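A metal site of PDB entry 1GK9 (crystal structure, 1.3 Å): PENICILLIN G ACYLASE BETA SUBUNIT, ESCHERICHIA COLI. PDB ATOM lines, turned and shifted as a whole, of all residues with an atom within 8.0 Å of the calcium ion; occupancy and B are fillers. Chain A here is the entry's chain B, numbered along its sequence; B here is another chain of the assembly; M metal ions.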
ATOM      1  N   GLY A  72      18.590   9.075 -18.799  1.00  0.00           N
ATOM      2  CA  GLY A  72      18.007  10.092 -17.922  1.00  0.00           C
ATOM      3  C   GLY A  72      19.069  11.094 -17.585  1.00  0.00           C
ATOM      4  O   GLY A  72      20.275  10.904 -17.811  1.00  0.00           O
ATOM      5  N   ASP A  73      18.687  12.244 -17.027  1.00  0.00           N
ATOM      6  CA  ASP A  73      19.635  13.298 -16.649  1.00  0.00           C
ATOM      7  C   ASP A  73      20.076  13.046 -15.211  1.00  0.00           C
ATOM      8  O   ASP A  73      19.434  13.528 -14.249  1.00  0.00           O
ATOM      9  CB  ASP A  73      19.033  14.675 -16.824  1.00  0.00           C
ATOM     10  CG  ASP A  73      20.073  15.742 -16.551  1.00  0.00           C
ATOM     11  OD1 ASP A  73      21.187  15.437 -16.050  1.00  0.00           O
ATOM     12  OD2 ASP A  73      19.797  16.943 -16.814  1.00  0.00           O
ATOM     13  N   ASP A  74      21.184  12.324 -15.068  1.00  0.00           N
ATOM     14  CA  ASP A  74      21.755  11.986 -13.763  1.00  0.00           C
ATOM     15  C   ASP A  74      23.090  12.696 -13.557  1.00  0.00           C
ATOM     16  O   ASP A  74      23.830  12.288 -12.652  1.00  0.00           O
ATOM     17  CB  ASP A  74      21.882  10.486 -13.586  1.00  0.00           C
ATOM     18  CG  ASP A  74      22.743   9.811 -14.629  1.00  0.00           C
ATOM     19  OD1 ASP A  74      23.152  10.441 -15.587  1.00  0.00           O
ATOM     20  OD2 ASP A  74      22.994   8.566 -14.438  1.00  0.00           O
ATOM     21  N   VAL A  75      23.425  13.719 -14.355  1.00  0.00           N
ATOM     22  CA  VAL A  75      24.700  14.408 -14.270  1.00  0.00           C
ATOM     23  C   VAL A  75      24.452  15.893 -14.438  1.00  0.00           C
ATOM     24  O   VAL A  75      23.840  16.350 -15.407  1.00  0.00           O
ATOM     25  CB  VAL A  75      25.679  13.934 -15.380  1.00  0.00           C
ATOM     26  CG1 VAL A  75      26.977  14.683 -15.288  1.00  0.00           C
ATOM     27  CG2 VAL A  75      25.964  12.447 -15.347  1.00  0.00           C
ATOM     28  N   ASP A  76      24.937  16.662 -13.442  1.00  0.00           N
ATOM     29  CA  ASP A  76      24.871  18.131 -13.486  1.00  0.00           C
ATOM     30  C   ASP A  76      26.277  18.696 -13.257  1.00  0.00           C
ATOM     31  O   ASP A  76      27.125  18.023 -12.644  1.00  0.00           O
ATOM     32  CB  ASP A  76      23.912  18.720 -12.457  1.00  0.00           C
ATOM     33  CG  ASP A  76      22.474  18.362 -12.602  1.00  0.00           C
ATOM     34  OD1 ASP A  76      22.020  17.939 -13.699  1.00  0.00           O
ATOM     35  OD2 ASP A  76      21.750  18.472 -11.590  1.00  0.00           O
ATOM     36  N   ILE A  77      26.526  19.882 -13.738  1.00  0.00           N
ATOM     37  CA  ILE A  77      27.797  20.580 -13.631  1.00  0.00           C
ATOM     38  C   ILE A  77      27.677  21.723 -12.638  1.00  0.00           C
ATOM     39  O   ILE A  77      26.862  22.627 -12.817  1.00  0.00           O
ATOM     40  CB  ILE A  77      28.189  21.198 -15.003  1.00  0.00           C
ATOM     41  CG1 ILE A  77      28.455  20.113 -16.034  1.00  0.00           C
ATOM     42  CG2 ILE A  77      29.395  22.133 -14.798  1.00  0.00           C
ATOM     43  CD1 ILE A  77      29.431  19.039 -15.653  1.00  0.00           C
ATOM     44  N   SER A 140      29.087  16.401 -11.354  1.00  0.00           N
ATOM     45  CA  SER A 140      28.426  15.616 -10.329  1.00  0.00           C
ATOM     46  C   SER A 140      27.451  14.587 -10.902  1.00  0.00           C
ATOM     47  O   SER A 140      26.435  14.885 -11.518  1.00  0.00           O
ATOM     48  CB  SER A 140      27.517  16.400  -9.393  1.00  0.00           C
ATOM     49  OG  SER A 140      28.104  17.468  -8.734  1.00  0.00           O
ATOM     50  N   PRO A 197      19.030  12.950  -8.914  1.00  0.00           N
ATOM     51  CA  PRO A 197      19.133  13.938  -7.835  1.00  0.00           C
ATOM     52  C   PRO A 197      17.830  14.591  -7.576  1.00  0.00           C
ATOM     53  O   PRO A 197      17.002  14.888  -8.426  1.00  0.00           O
ATOM     54  CB  PRO A 197      20.152  14.941  -8.394  1.00  0.00           C
ATOM     55  CG  PRO A 197      19.966  14.906  -9.888  1.00  0.00           C
ATOM     56  CD  PRO A 197      19.569  13.456 -10.193  1.00  0.00           C
ATOM     57  N   ARG A 199      16.663  17.948  -6.886  1.00  0.00           N
ATOM     58  CA  ARG A 199      17.239  19.248  -7.154  1.00  0.00           C
ATOM     59  C   ARG A 199      16.471  20.339  -6.389  1.00  0.00           C
ATOM     60  O   ARG A 199      15.246  20.234  -6.238  1.00  0.00           O
ATOM     61  CB  ARG A 199      17.231  19.529  -8.665  1.00  0.00           C
ATOM     62  CG  ARG A 199      18.064  18.506  -9.442  1.00  0.00           C
ATOM     63  CD  ARG A 199      18.070  18.854 -10.915  1.00  0.00           C
ATOM     64  NE  ARG A 199      19.017  18.061 -11.735  1.00  0.00           N
ATOM     65  CZ  ARG A 199      18.681  16.932 -12.369  1.00  0.00           C
ATOM     66  NH1 ARG A 199      17.495  16.407 -12.268  1.00  0.00           N
ATOM     67  NH2 ARG A 199      19.623  16.385 -13.121  1.00  0.00           N
ATOM     68  N   HIS A 203      16.061  24.856 -10.169  1.00  0.00           N
ATOM     69  CA  HIS A 203      17.225  24.297 -10.867  1.00  0.00           C
ATOM     70  C   HIS A 203      16.881  23.720 -12.262  1.00  0.00           C
ATOM     71  O   HIS A 203      16.229  22.685 -12.330  1.00  0.00           O
ATOM     72  CB  HIS A 203      17.874  23.252  -9.980  1.00  0.00           C
ATOM     73  CG  HIS A 203      19.096  22.549 -10.489  1.00  0.00           C
ATOM     74  ND1 HIS A 203      19.847  21.773  -9.641  1.00  0.00           N
ATOM     75  CD2 HIS A 203      19.644  22.440 -11.734  1.00  0.00           C
ATOM     76  CE1 HIS A 203      20.839  21.231 -10.342  1.00  0.00           C
ATOM     77  NE2 HIS A 203      20.730  21.601 -11.624  1.00  0.00           N
ATOM     78  N   ASP A 204      17.290  24.435 -13.293  1.00  0.00           N
ATOM     79  CA  ASP A 204      17.096  23.933 -14.697  1.00  0.00           C
ATOM     80  C   ASP A 204      18.210  22.916 -14.962  1.00  0.00           C
ATOM     81  O   ASP A 204      19.356  23.288 -15.012  1.00  0.00           O
ATOM     82  CB  ASP A 204      17.156  25.124 -15.609  1.00  0.00           C
ATOM     83  CG  ASP A 204      16.902  24.809 -17.077  1.00  0.00           C
ATOM     84  OD1 ASP A 204      17.143  23.645 -17.516  1.00  0.00           O
ATOM     85  OD2 ASP A 204      16.476  25.744 -17.788  1.00  0.00           O
ATOM     86  N   PRO A 205      17.841  21.655 -15.100  1.00  0.00           N
ATOM     87  CA  PRO A 205      18.858  20.580 -15.177  1.00  0.00           C
ATOM     88  C   PRO A 205      19.654  20.524 -16.446  1.00  0.00           C
ATOM     89  O   PRO A 205      20.578  19.727 -16.582  1.00  0.00           O
ATOM     90  CB  PRO A 205      18.078  19.269 -14.938  1.00  0.00           C
ATOM     91  CG  PRO A 205      16.725  19.621 -15.567  1.00  0.00           C
ATOM     92  CD  PRO A 205      16.505  21.085 -15.139  1.00  0.00           C
ATOM     93  N   ARG A 206      19.360  21.401 -17.423  1.00  0.00           N
ATOM     94  CA  ARG A 206      20.101  21.475 -18.653  1.00  0.00           C
ATOM     95  C   ARG A 206      21.306  22.359 -18.588  1.00  0.00           C
ATOM     96  O   ARG A 206      22.073  22.386 -19.575  1.00  0.00           O
ATOM     97  CB  ARG A 206      19.190  22.015 -19.782  1.00  0.00           C
ATOM     98  CG  ARG A 206      17.951  21.161 -19.983  1.00  0.00           C
ATOM     99  CD  ARG A 206      16.945  21.878 -20.864  1.00  0.00           C
ATOM    100  NE  ARG A 206      16.432  23.109 -20.239  1.00  0.00           N
ATOM    101  CZ  ARG A 206      15.594  23.909 -20.801  1.00  0.00           C
ATOM    102  NH1 ARG A 206      15.068  23.655 -21.983  1.00  0.00           N
ATOM    103  NH2 ARG A 206      15.191  25.016 -20.186  1.00  0.00           N
ATOM    104  N   LEU A 207      21.474  23.114 -17.506  1.00  0.00           N
ATOM    105  CA  LEU A 207      22.502  24.164 -17.419  1.00  0.00           C
ATOM    106  C   LEU A 207      23.228  24.139 -16.084  1.00  0.00           C
ATOM    107  O   LEU A 207      22.640  23.655 -15.105  1.00  0.00           O
ATOM    108  CB  LEU A 207      21.767  25.518 -17.620  1.00  0.00           C
ATOM    109  CG  LEU A 207      21.113  25.702 -18.982  1.00  0.00           C
ATOM    110  CD1 LEU A 207      20.001  26.755 -18.965  1.00  0.00           C
ATOM    111  CD2 LEU A 207      22.136  26.045 -20.040  1.00  0.00           C
ATOM    112  N   PRO A 208      24.454  24.623 -16.044  1.00  0.00           N
ATOM    113  CA  PRO A 208      25.249  24.503 -14.811  1.00  0.00           C
ATOM    114  C   PRO A 208      24.630  25.230 -13.634  1.00  0.00           C
ATOM    115  O   PRO A 208      23.829  26.154 -13.814  1.00  0.00           O
ATOM    116  CB  PRO A 208      26.616  25.066 -15.150  1.00  0.00           C
ATOM    117  CG  PRO A 208      26.669  24.994 -16.666  1.00  0.00           C
ATOM    118  CD  PRO A 208      25.224  25.217 -17.119  1.00  0.00           C
ATOM    119  N   VAL A 209      24.991  24.826 -12.425  1.00  0.00           N
ATOM    120  CA  VAL A 209      24.474  25.437 -11.214  1.00  0.00           C
ATOM    121  C   VAL A 209      25.670  26.005 -10.454  1.00  0.00           C
ATOM    122  O   VAL A 209      26.753  25.411 -10.413  1.00  0.00           O
ATOM    123  CB  VAL A 209      23.741  24.421 -10.302  1.00  0.00           C
ATOM    124  CG1 VAL A 209      22.235  24.473 -10.544  1.00  0.00           C
ATOM    125  CG2 VAL A 209      24.185  22.965 -10.511  1.00  0.00           C
ATOM    126  N   TRP A 217      22.435  19.659  -4.579  1.00  0.00           N
ATOM    127  CA  TRP A 217      21.334  18.746  -4.553  1.00  0.00           C
ATOM    128  C   TRP A 217      20.854  18.508  -3.121  1.00  0.00           C
ATOM    129  O   TRP A 217      21.702  18.448  -2.221  1.00  0.00           O
ATOM    130  CB  TRP A 217      21.811  17.414  -5.159  1.00  0.00           C
ATOM    131  CG  TRP A 217      22.109  17.400  -6.627  1.00  0.00           C
ATOM    132  CD1 TRP A 217      21.713  18.308  -7.566  1.00  0.00           C
ATOM    133  CD2 TRP A 217      22.924  16.441  -7.289  1.00  0.00           C
ATOM    134  NE1 TRP A 217      22.175  17.932  -8.810  1.00  0.00           N
ATOM    135  CE2 TRP A 217      22.911  16.761  -8.639  1.00  0.00           C
ATOM    136  CE3 TRP A 217      23.610  15.284  -6.867  1.00  0.00           C
ATOM    137  CZ2 TRP A 217      23.565  16.009  -9.616  1.00  0.00           C
ATOM    138  CZ3 TRP A 217      24.245  14.552  -7.832  1.00  0.00           C
ATOM    139  CH2 TRP A 217      24.211  14.883  -9.185  1.00  0.00           C
ATOM    140  N   ALA A 250      14.727  13.872 -20.498  1.00  0.00           N
ATOM    141  CA  ALA A 250      15.911  13.253 -21.045  1.00  0.00           C
ATOM    142  C   ALA A 250      17.219  13.831 -20.501  1.00  0.00           C
ATOM    143  O   ALA A 250      17.253  14.915 -19.921  1.00  0.00           O
ATOM    144  CB  ALA A 250      15.905  13.542 -22.541  1.00  0.00           C
ATOM    145  N   SER A 251      18.325  13.096 -20.774  1.00  0.00           N
ATOM    146  CA  SER A 251      19.690  13.584 -20.717  1.00  0.00           C
ATOM    147  C   SER A 251      19.731  15.048 -21.206  1.00  0.00           C
ATOM    148  O   SER A 251      19.062  15.417 -22.159  1.00  0.00           O
ATOM    149  CB  SER A 251      20.465  12.730 -21.732  1.00  0.00           C
ATOM    150  OG  SER A 251      21.807  13.198 -21.830  1.00  0.00           O
ATOM    151  N   ASP A 252      20.640  15.797 -20.593  1.00  0.00           N
ATOM    152  CA  ASP A 252      20.811  17.182 -21.013  1.00  0.00           C
ATOM    153  C   ASP A 252      21.690  17.372 -22.247  1.00  0.00           C
ATOM    154  O   ASP A 252      21.812  18.511 -22.713  1.00  0.00           O
ATOM    155  CB  ASP A 252      21.366  18.007 -19.837  1.00  0.00           C
ATOM    156  CG  ASP A 252      22.767  17.616 -19.411  1.00  0.00           C
ATOM    157  OD1 ASP A 252      23.602  17.426 -20.330  1.00  0.00           O
ATOM    158  OD2 ASP A 252      23.053  17.556 -18.196  1.00  0.00           O
ATOM    159  N   LEU A 253      22.130  16.293 -22.858  1.00  0.00           N
ATOM    160  CA  LEU A 253      22.953  16.433 -24.074  1.00  0.00           C
ATOM    161  C   LEU A 253      22.194  17.182 -25.131  1.00  0.00           C
ATOM    162  O   LEU A 253      21.028  16.816 -25.472  1.00  0.00           O
ATOM    163  CB  LEU A 253      23.280  15.043 -24.620  1.00  0.00           C
ATOM    164  CG  LEU A 253      24.266  14.181 -23.811  1.00  0.00           C
ATOM    165  CD1 LEU A 253      24.237  12.813 -24.498  1.00  0.00           C
ATOM    166  CD2 LEU A 253      25.642  14.812 -23.803  1.00  0.00           C
ATOM    167  N   SER B 149      26.838  11.164 -19.184  1.00  0.00           N
ATOM    168  CA  SER B 149      26.549  12.069 -20.281  1.00  0.00           C
ATOM    169  C   SER B 149      26.040  13.457 -19.910  1.00  0.00           C
ATOM    170  O   SER B 149      24.932  13.526 -19.427  1.00  0.00           O
ATOM    171  CB  SER B 149      25.463  11.438 -21.211  1.00  0.00           C
ATOM    172  OG  SER B 149      25.909  10.315 -21.919  1.00  0.00           O
ATOM    173  N   THR B 150      26.824  14.536 -20.130  1.00  0.00           N
ATOM    174  CA  THR B 150      26.315  15.893 -19.898  1.00  0.00           C
ATOM    175  C   THR B 150      26.929  16.811 -20.928  1.00  0.00           C
ATOM    176  O   THR B 150      28.050  16.549 -21.384  1.00  0.00           O
ATOM    177  CB  THR B 150      26.539  16.404 -18.483  1.00  0.00           C
ATOM    178  OG1 THR B 150      25.887  17.681 -18.336  1.00  0.00           O
ATOM    179  CG2 THR B 150      28.020  16.619 -18.161  1.00  0.00           C
ATOM    180  N   SER B 151      26.213  17.857 -21.340  1.00  0.00           N
ATOM    181  CA  SER B 151      26.753  18.888 -22.209  1.00  0.00           C
ATOM    182  C   SER B 151      26.371  20.245 -21.593  1.00  0.00           C
ATOM    183  O   SER B 151      26.331  21.240 -22.362  1.00  0.00           O
ATOM    184  CB  SER B 151      26.328  18.819 -23.672  1.00  0.00           C
ATOM    185  OG  SER B 151      24.931  19.001 -23.827  1.00  0.00           O
ATOM    186  N   GLU B 152      26.234  20.374 -20.276  1.00  0.00           N
ATOM    187  CA  GLU B 152      25.754  21.629 -19.726  1.00  0.00           C
ATOM    188  C   GLU B 152      26.607  22.852 -20.038  1.00  0.00           C
ATOM    189  O   GLU B 152      26.017  23.955 -20.177  1.00  0.00           O
ATOM    190  CB  GLU B 152      25.582  21.525 -18.206  1.00  0.00           C
ATOM    191  CG  GLU B 152      24.449  20.578 -17.805  1.00  0.00           C
ATOM    192  CD  GLU B 152      24.248  20.485 -16.294  1.00  0.00           C
ATOM    193  OE1 GLU B 152      24.949  21.265 -15.586  1.00  0.00           O
ATOM    194  OE2 GLU B 152      23.402  19.676 -15.860  1.00  0.00           O
ATOM    195  N   ASN B 155      25.714  23.742 -23.457  1.00  0.00           N
ATOM    196  CA  ASN B 155      24.331  24.235 -23.477  1.00  0.00           C
ATOM    197  C   ASN B 155      24.317  25.702 -23.056  1.00  0.00           C
ATOM    198  O   ASN B 155      23.546  26.489 -23.607  1.00  0.00           O
ATOM    199  CB  ASN B 155      23.452  23.375 -22.570  1.00  0.00           C
ATOM    200  CG  ASN B 155      23.322  21.924 -22.998  1.00  0.00           C
ATOM    201  OD1 ASN B 155      23.774  21.536 -24.063  1.00  0.00           O
ATOM    202  ND2 ASN B 155      22.708  21.155 -22.100  1.00  0.00           N
HETATM  203 CA    CA M   1      22.057  17.833 -16.067  1.00  0.00          CA
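The calcium ion is bound by the side-chain carboxylate (OE2) of Glu 152 of chain B (2.3 Å), the side-chain carboxylate (OD2) of Asp 252 (2.4 Å), the side-chain carboxylate (OD1) of Asp 76 (2.4 Å), the backbone carbonyl oxygen (O) of Val 75 (2.4 Å), the backbone carbonyl oxygen (O) of Pro 205 (2.5 Å), the side-chain carboxylate (OD2) of Asp 73 (2.5 Å) and the side-chain carboxylate (OD1) of Asp 73 (2.5 Å). The calcium ion has seven donor atoms within binding distance.
Of the 26 residues printed, 6 come within 4 Å of the calcium ion. The nearest printed residue that does not touch the calcium ion is Arg 199 (4.1 Å).
OG1 of Thr 150 of chain B lies close to N of Glu 152 of chain B, 3.3 Å away. OG1 of Thr 150 of chain B sits at hydrogen-bond distance from OD1 of Asp 252, 3.0 Å away. The backbone carbonyl oxygen of Asp 252 lies within hydrogen-bond range of the side-chain amide nitrogen of Asn 155 of chain B. The guanidinium group (NE) of Arg 199 is in salt-bridge range of the side-chain carboxylate (OD2) of Asp 76 (2.8 Å). OD2 of Asp 76 sits close to NE2 of His 203, 3.3 Å away. The side-chain carboxylate of Asp 76 sits at hydrogen-bond distance from the indole nitrogen of Trp 217, at 2.9 Å. The backbone carbonyl oxygen (O) of Asp 76 lies within hydrogen-bond range of the backbone NH (N) of Ser 140. O of Asp 73 sits at hydrogen-bond distance from NH2 of Arg 199 (3.1 Å).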
